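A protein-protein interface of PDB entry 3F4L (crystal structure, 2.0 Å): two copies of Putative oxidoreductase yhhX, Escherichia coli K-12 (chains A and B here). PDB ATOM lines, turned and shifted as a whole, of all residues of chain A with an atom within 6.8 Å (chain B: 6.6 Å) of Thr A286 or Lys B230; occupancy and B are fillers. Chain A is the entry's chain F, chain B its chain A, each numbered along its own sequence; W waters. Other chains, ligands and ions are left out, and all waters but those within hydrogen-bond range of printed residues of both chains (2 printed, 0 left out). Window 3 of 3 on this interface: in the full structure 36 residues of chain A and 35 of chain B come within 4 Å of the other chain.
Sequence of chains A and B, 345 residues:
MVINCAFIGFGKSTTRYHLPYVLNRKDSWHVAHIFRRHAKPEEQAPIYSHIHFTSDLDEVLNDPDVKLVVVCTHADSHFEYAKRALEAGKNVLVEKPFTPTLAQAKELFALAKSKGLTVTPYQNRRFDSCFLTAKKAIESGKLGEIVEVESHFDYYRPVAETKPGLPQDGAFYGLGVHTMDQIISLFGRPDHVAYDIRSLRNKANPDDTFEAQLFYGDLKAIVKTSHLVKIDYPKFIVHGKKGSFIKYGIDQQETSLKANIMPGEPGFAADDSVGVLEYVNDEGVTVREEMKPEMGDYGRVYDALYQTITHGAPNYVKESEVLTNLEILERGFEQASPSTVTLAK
No position is printed for both chains. Of the 11 pairs that touch across the chains among the printed residues, none has its exchanged pair printed and touching as well.
The side-chain hydroxyl (OG1) of Thr A286 is in hydrogen-bond range of the side-chain amino group (NZ) of Lys B230, at 3.1 Å. The backbone NH (N) of Lys B230 sits at hydrogen-bond distance from the side-chain hydroxyl (OG) of Ser A244, 3.2 Å away. The backbone NH of Ile B231 is in hydrogen-bond range of the side-chain hydroxyl of Ser A244, 3.3 Å away.
Of the 15 printed residues of chain A, 7 touch a printed residue of chain B. Hydrophobic or aromatic side chains of chain A within 4 Å of the printed part of chain B: His A239 and Val A280. Hydrophobic or aromatic side chains of chain B that line the printed part of chain A: Tyr B156, Val B229 and Ile B231. Among the printed residues, no Asp or Glu carboxylate lies within 4 Å of a Lys or Arg side-chain nitrogen of the other chain.
Among the printed residues, pairs that only touch across the chains: Glu A278 with Lys B230, Lys A242 with Tyr B156, His A239 with Ile B231, Glu A278 with Ile B231, His A239 with Val B229, His A239 with Leu B228, Gly A243 with Lys B230 and Val A280 with Lys B230.
Water W2 lies within hydrogen-bond range of O of Ile B231 (2.7 Å) and NE2 of His A239 (3.1 Å). Water W1 lies within hydrogen-bond range of the backbone carbonyl oxygen of Leu B228 (2.7 Å), the backbone NH of Lys B230 (2.8 Å), the side-chain hydroxyl of Ser A244 (3.0 Å), the backbone carbonyl oxygen of Gly A240 (3.2 Å) and the backbone NH of Val B229 (3.4 Å).
Printed residues of chain B within 4 Å of His A239: Leu B228 (3.9 Å), Val B229 (3.8 Å) and Ile B231 (3.5 Å). Of chain B, only Lys B230 comes within 4 Å of Thr A286. Of the printed residues of chain A, Leu B228 touches His A239. Of chain A, only Gly A243, Ser A244, Glu A278, Val A280 and Thr A286 come within 4 Å of Lys B230. The nearest residue of chain B that does not touch Thr A286 is Tyr B156 (6.3 Å). The nearest residue of chain A that does not touch Lys B230 is His A239 (4.4 Å).
OG of Ser A244 sits at hydrogen-bond distance from ND1 of His A239, at 2.5 Å. N of Leu B228 sits at hydrogen-bond distance from O of Tyr B155, at 3.3 Å. The backbone NH (N) of Ser A244 lies within hydrogen-bond range of the backbone carbonyl oxygen (O) of Glu A278. The backbone NH (N) of Val A280 sits at hydrogen-bond distance from the backbone carbonyl oxygen (O) of Lys A242, at 3.0 Å. The backbone NH (N) of Val B229 sits at hydrogen-bond distance from the backbone carbonyl oxygen (O) of Tyr B155 (3.0 Å). NH1 of Arg A288 is in salt-bridge range of OE1 of Glu A278, at 2.6 Å.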
ATOM      1  N   HIS A 239      19.743  24.073  10.894  1.00  0.00           N
ATOM      2  CA  HIS A 239      18.655  24.308  11.827  1.00  0.00           C
ATOM      3  C   HIS A 239      18.895  25.615  12.589  1.00  0.00           C
ATOM      4  O   HIS A 239      19.996  25.872  13.101  1.00  0.00           O
ATOM      5  CB  HIS A 239      18.518  23.145  12.818  1.00  0.00           C
ATOM      6  CG  HIS A 239      18.011  21.877  12.201  1.00  0.00           C
ATOM      7  ND1 HIS A 239      16.830  21.808  11.492  1.00  0.00           N
ATOM      8  CD2 HIS A 239      18.527  20.626  12.190  1.00  0.00           C
ATOM      9  CE1 HIS A 239      16.642  20.572  11.070  1.00  0.00           C
ATOM     10  NE2 HIS A 239      17.658  19.834  11.481  1.00  0.00           N
ATOM     11  N   GLY A 240      17.853  26.440  12.624  1.00  0.00           N
ATOM     12  CA  GLY A 240      17.894  27.714  13.315  1.00  0.00           C
ATOM     13  C   GLY A 240      16.666  27.781  14.207  1.00  0.00           C
ATOM     14  O   GLY A 240      15.775  26.935  14.106  1.00  0.00           O
ATOM     15  N   LYS A 242      14.163  29.657  14.076  1.00  0.00           N
ATOM     16  CA  LYS A 242      12.942  29.951  13.343  1.00  0.00           C
ATOM     17  C   LYS A 242      12.648  28.973  12.208  1.00  0.00           C
ATOM     18  O   LYS A 242      11.554  28.990  11.647  1.00  0.00           O
ATOM     19  CB  LYS A 242      13.002  31.374  12.775  1.00  0.00           C
ATOM     20  CG  LYS A 242      13.314  32.457  13.803  1.00  0.00           C
ATOM     21  CD  LYS A 242      13.356  33.838  13.140  1.00  0.00           C
ATOM     22  CE  LYS A 242      14.012  34.893  14.029  1.00  0.00           C
ATOM     23  NZ  LYS A 242      13.277  35.116  15.303  1.00  0.00           N
ATOM     24  N   GLY A 243      13.608  28.122  11.861  1.00  0.00           N
ATOM     25  CA  GLY A 243      13.351  27.187  10.784  1.00  0.00           C
ATOM     26  C   GLY A 243      14.515  26.318  10.359  1.00  0.00           C
ATOM     27  O   GLY A 243      15.618  26.419  10.895  1.00  0.00           O
ATOM     28  N   SER A 244      14.254  25.471   9.371  1.00  0.00           N
ATOM     29  CA  SER A 244      15.246  24.542   8.857  1.00  0.00           C
ATOM     30  C   SER A 244      15.432  24.652   7.350  1.00  0.00           C
ATOM     31  O   SER A 244      14.524  25.065   6.627  1.00  0.00           O
ATOM     32  CB  SER A 244      14.833  23.105   9.179  1.00  0.00           C
ATOM     33  OG  SER A 244      14.771  22.873  10.573  1.00  0.00           O
ATOM     34  N   PHE A 245      16.621  24.261   6.904  1.00  0.00           N
ATOM     35  CA  PHE A 245      17.001  24.234   5.494  1.00  0.00           C
ATOM     36  C   PHE A 245      17.578  22.842   5.233  1.00  0.00           C
ATOM     37  O   PHE A 245      18.454  22.392   5.974  1.00  0.00           O
ATOM     38  CB  PHE A 245      18.101  25.258   5.194  1.00  0.00           C
ATOM     39  CG  PHE A 245      18.729  25.094   3.823  1.00  0.00           C
ATOM     40  CD1 PHE A 245      18.074  25.542   2.680  1.00  0.00           C
ATOM     41  CD2 PHE A 245      19.969  24.480   3.682  1.00  0.00           C
ATOM     42  CE1 PHE A 245      18.643  25.382   1.422  1.00  0.00           C
ATOM     43  CE2 PHE A 245      20.553  24.315   2.422  1.00  0.00           C
ATOM     44  CZ  PHE A 245      19.888  24.767   1.288  1.00  0.00           C
ATOM     45  N   GLU A 278      11.897  25.612   5.392  1.00  0.00           N
ATOM     46  CA  GLU A 278      10.647  25.724   6.131  1.00  0.00           C
ATOM     47  C   GLU A 278      10.918  26.538   7.381  1.00  0.00           C
ATOM     48  O   GLU A 278      11.712  26.136   8.244  1.00  0.00           O
ATOM     49  CB  GLU A 278      10.088  24.357   6.525  1.00  0.00           C
ATOM     50  CG  GLU A 278       8.674  24.462   7.089  1.00  0.00           C
ATOM     51  CD  GLU A 278       8.007  23.118   7.302  1.00  0.00           C
ATOM     52  OE1 GLU A 278       8.011  22.291   6.369  1.00  0.00           O
ATOM     53  OE2 GLU A 278       7.464  22.896   8.402  1.00  0.00           O
ATOM     54  N   TYR A 279      10.247  27.681   7.474  1.00  0.00           N
ATOM     55  CA  TYR A 279      10.430  28.583   8.593  1.00  0.00           C
ATOM     56  C   TYR A 279       9.148  29.321   8.957  1.00  0.00           C
ATOM     57  O   TYR A 279       8.143  29.248   8.246  1.00  0.00           O
ATOM     58  CB  TYR A 279      11.510  29.606   8.243  1.00  0.00           C
ATOM     59  CG  TYR A 279      11.126  30.500   7.080  1.00  0.00           C
ATOM     60  CD1 TYR A 279      11.014  29.987   5.785  1.00  0.00           C
ATOM     61  CD2 TYR A 279      10.839  31.849   7.284  1.00  0.00           C
ATOM     62  CE1 TYR A 279      10.620  30.796   4.721  1.00  0.00           C
ATOM     63  CE2 TYR A 279      10.442  32.669   6.228  1.00  0.00           C
ATOM     64  CZ  TYR A 279      10.334  32.134   4.951  1.00  0.00           C
ATOM     65  OH  TYR A 279       9.925  32.935   3.912  1.00  0.00           O
ATOM     66  N   VAL A 280       9.215  30.047  10.069  1.00  0.00           N
ATOM     67  CA  VAL A 280       8.102  30.834  10.581  1.00  0.00           C
ATOM     68  C   VAL A 280       8.437  32.298  10.286  1.00  0.00           C
ATOM     69  O   VAL A 280       9.424  32.826  10.797  1.00  0.00           O
ATOM     70  CB  VAL A 280       7.958  30.635  12.110  1.00  0.00           C
ATOM     71  CG1 VAL A 280       6.778  31.436  12.646  1.00  0.00           C
ATOM     72  CG2 VAL A 280       7.781  29.157  12.426  1.00  0.00           C
ATOM     73  N   ASN A 281       7.627  32.948   9.457  1.00  0.00           N
ATOM     74  CA  ASN A 281       7.876  34.346   9.102  1.00  0.00           C
ATOM     75  C   ASN A 281       7.485  35.321  10.208  1.00  0.00           C
ATOM     76  O   ASN A 281       6.891  34.925  11.213  1.00  0.00           O
ATOM     77  CB  ASN A 281       7.140  34.703   7.801  1.00  0.00           C
ATOM     78  CG  ASN A 281       5.629  34.538   7.905  1.00  0.00           C
ATOM     79  OD1 ASN A 281       4.957  34.341   6.894  1.00  0.00           O
ATOM     80  ND2 ASN A 281       5.088  34.632   9.117  1.00  0.00           N
ATOM     81  N   GLY A 284       4.388  35.090  12.043  1.00  0.00           N
ATOM     82  CA  GLY A 284       4.170  33.856  12.778  1.00  0.00           C
ATOM     83  C   GLY A 284       3.571  32.718  11.969  1.00  0.00           C
ATOM     84  O   GLY A 284       3.140  31.712  12.537  1.00  0.00           O
ATOM     85  N   VAL A 285       3.544  32.863  10.648  1.00  0.00           N
ATOM     86  CA  VAL A 285       2.988  31.824   9.783  1.00  0.00           C
ATOM     87  C   VAL A 285       4.093  30.925   9.230  1.00  0.00           C
ATOM     88  O   VAL A 285       5.123  31.414   8.765  1.00  0.00           O
ATOM     89  CB  VAL A 285       2.205  32.445   8.599  1.00  0.00           C
ATOM     90  CG1 VAL A 285       1.629  31.347   7.724  1.00  0.00           C
ATOM     91  CG2 VAL A 285       1.082  33.336   9.128  1.00  0.00           C
ATOM     92  N   THR A 286       3.884  29.611   9.286  1.00  0.00           N
ATOM     93  CA  THR A 286       4.883  28.673   8.779  1.00  0.00           C
ATOM     94  C   THR A 286       4.872  28.640   7.254  1.00  0.00           C
ATOM     95  O   THR A 286       3.851  28.337   6.630  1.00  0.00           O
ATOM     96  CB  THR A 286       4.646  27.245   9.310  1.00  0.00           C
ATOM     97  OG1 THR A 286       4.795  27.232  10.734  1.00  0.00           O
ATOM     98  CG2 THR A 286       5.651  26.283   8.706  1.00  0.00           C
ATOM     99  N   VAL A 287       6.022  28.954   6.666  1.00  0.00           N
ATOM    100  CA  VAL A 287       6.186  28.987   5.215  1.00  0.00           C
ATOM    101  C   VAL A 287       7.198  27.937   4.753  1.00  0.00           C
ATOM    102  O   VAL A 287       8.175  27.658   5.448  1.00  0.00           O
ATOM    103  CB  VAL A 287       6.681  30.389   4.752  1.00  0.00           C
ATOM    104  CG1 VAL A 287       6.872  30.415   3.243  1.00  0.00           C
ATOM    105  CG2 VAL A 287       5.679  31.458   5.175  1.00  0.00           C
ATOM    106  N   ARG A 288       6.952  27.351   3.583  1.00  0.00           N
ATOM    107  CA  ARG A 288       7.865  26.354   3.022  1.00  0.00           C
ATOM    108  C   ARG A 288       8.210  26.793   1.606  1.00  0.00           C
ATOM    109  O   ARG A 288       7.318  27.016   0.787  1.00  0.00           O
ATOM    110  CB  ARG A 288       7.217  24.966   2.995  1.00  0.00           C
ATOM    111  CG  ARG A 288       8.189  23.832   2.664  1.00  0.00           C
ATOM    112  CD  ARG A 288       7.458  22.503   2.566  1.00  0.00           C
ATOM    113  NE  ARG A 288       8.327  21.378   2.222  1.00  0.00           N
ATOM    114  CZ  ARG A 288       8.920  20.581   3.108  1.00  0.00           C
ATOM    115  NH1 ARG A 288       8.751  20.776   4.409  1.00  0.00           N
ATOM    116  NH2 ARG A 288       9.670  19.570   2.688  1.00  0.00           N
ATOM    117  N   TYR B 155      11.622  17.847  18.352  1.00  0.00           N
ATOM    118  CA  TYR B 155      10.395  18.656  18.342  1.00  0.00           C
ATOM    119  C   TYR B 155      10.729  20.023  17.779  1.00  0.00           C
ATOM    120  O   TYR B 155      11.896  20.371  17.601  1.00  0.00           O
ATOM    121  CB  TYR B 155       9.886  18.951  19.759  1.00  0.00           C
ATOM    122  CG  TYR B 155       9.537  17.769  20.622  1.00  0.00           C
ATOM    123  CD1 TYR B 155       8.332  17.089  20.454  1.00  0.00           C
ATOM    124  CD2 TYR B 155      10.399  17.354  21.638  1.00  0.00           C
ATOM    125  CE1 TYR B 155       7.987  16.028  21.282  1.00  0.00           C
ATOM    126  CE2 TYR B 155      10.063  16.289  22.474  1.00  0.00           C
ATOM    127  CZ  TYR B 155       8.857  15.635  22.289  1.00  0.00           C
ATOM    128  OH  TYR B 155       8.514  14.580  23.108  1.00  0.00           O
ATOM    129  N   TYR B 156       9.685  20.801  17.513  1.00  0.00           N
ATOM    130  CA  TYR B 156       9.873  22.189  17.124  1.00  0.00           C
ATOM    131  C   TYR B 156       8.958  22.932  18.089  1.00  0.00           C
ATOM    132  O   TYR B 156       7.773  23.135  17.808  1.00  0.00           O
ATOM    133  CB  TYR B 156       9.470  22.519  15.683  1.00  0.00           C
ATOM    134  CG  TYR B 156       9.782  23.984  15.411  1.00  0.00           C
ATOM    135  CD1 TYR B 156      11.109  24.424  15.314  1.00  0.00           C
ATOM    136  CD2 TYR B 156       8.768  24.943  15.385  1.00  0.00           C
ATOM    137  CE1 TYR B 156      11.418  25.787  15.207  1.00  0.00           C
ATOM    138  CE2 TYR B 156       9.061  26.308  15.274  1.00  0.00           C
ATOM    139  CZ  TYR B 156      10.388  26.721  15.188  1.00  0.00           C
ATOM    140  OH  TYR B 156      10.677  28.061  15.076  1.00  0.00           O
ATOM    141  N   LEU B 228      14.411  22.259  18.564  1.00  0.00           N
ATOM    142  CA  LEU B 228      14.474  23.238  17.480  1.00  0.00           C
ATOM    143  C   LEU B 228      14.736  22.587  16.123  1.00  0.00           C
ATOM    144  O   LEU B 228      15.735  22.869  15.473  1.00  0.00           O
ATOM    145  CB  LEU B 228      15.559  24.274  17.790  1.00  0.00           C
ATOM    146  CG  LEU B 228      15.306  25.128  19.037  1.00  0.00           C
ATOM    147  CD1 LEU B 228      16.541  25.962  19.345  1.00  0.00           C
ATOM    148  CD2 LEU B 228      14.079  26.025  18.803  1.00  0.00           C
ATOM    149  N   VAL B 229      13.819  21.720  15.709  1.00  0.00           N
ATOM    150  CA  VAL B 229      13.936  21.011  14.442  1.00  0.00           C
ATOM    151  C   VAL B 229      12.630  21.181  13.671  1.00  0.00           C
ATOM    152  O   VAL B 229      11.662  20.461  13.894  1.00  0.00           O
ATOM    153  CB  VAL B 229      14.232  19.503  14.686  1.00  0.00           C
ATOM    154  CG1 VAL B 229      14.220  18.719  13.373  1.00  0.00           C
ATOM    155  CG2 VAL B 229      15.574  19.357  15.374  1.00  0.00           C
ATOM    156  N   LYS B 230      12.611  22.152  12.767  1.00  0.00           N
ATOM    157  CA  LYS B 230      11.421  22.428  11.973  1.00  0.00           C
ATOM    158  C   LYS B 230      11.178  21.334  10.944  1.00  0.00           C
ATOM    159  O   LYS B 230      10.042  20.947  10.701  1.00  0.00           O
ATOM    160  CB  LYS B 230      11.555  23.789  11.293  1.00  0.00           C
ATOM    161  CG  LYS B 230      10.260  24.293  10.675  1.00  0.00           C
ATOM    162  CD  LYS B 230       9.160  24.453  11.734  1.00  0.00           C
ATOM    163  CE  LYS B 230       7.913  25.097  11.131  1.00  0.00           C
ATOM    164  NZ  LYS B 230       6.835  25.346  12.124  1.00  0.00           N
ATOM    165  N   ILE B 231      12.244  20.835  10.329  1.00  0.00           N
ATOM    166  CA  ILE B 231      12.107  19.754   9.355  1.00  0.00           C
ATOM    167  C   ILE B 231      12.763  18.520   9.971  1.00  0.00           C
ATOM    168  O   ILE B 231      13.986  18.463  10.106  1.00  0.00           O
ATOM    169  CB  ILE B 231      12.815  20.075   8.027  1.00  0.00           C
ATOM    170  CG1 ILE B 231      12.152  21.279   7.349  1.00  0.00           C
ATOM    171  CG2 ILE B 231      12.739  18.855   7.113  1.00  0.00           C
ATOM    172  CD1 ILE B 231      12.900  21.764   6.116  1.00  0.00           C
ATOM    173  N   ASP B 232      11.944  17.540  10.338  1.00  0.00           N
ATOM    174  CA  ASP B 232      12.426  16.326  10.985  1.00  0.00           C
ATOM    175  C   ASP B 232      13.448  15.476  10.246  1.00  0.00           C
ATOM    176  O   ASP B 232      13.474  15.419   9.016  1.00  0.00           O
ATOM    177  CB  ASP B 232      11.251  15.417  11.363  1.00  0.00           C
ATOM    178  CG  ASP B 232      10.617  15.799  12.691  1.00  0.00           C
ATOM    179  OD1 ASP B 232      11.365  16.090  13.647  1.00  0.00           O
ATOM    180  OD2 ASP B 232       9.375  15.798  12.785  1.00  0.00           O
HETATM  181  O   HOH W   1      14.613  24.090  13.359  1.00  0.00           O
HETATM  182  O   HOH W   2      16.425  17.413   9.965  1.00  0.00           O
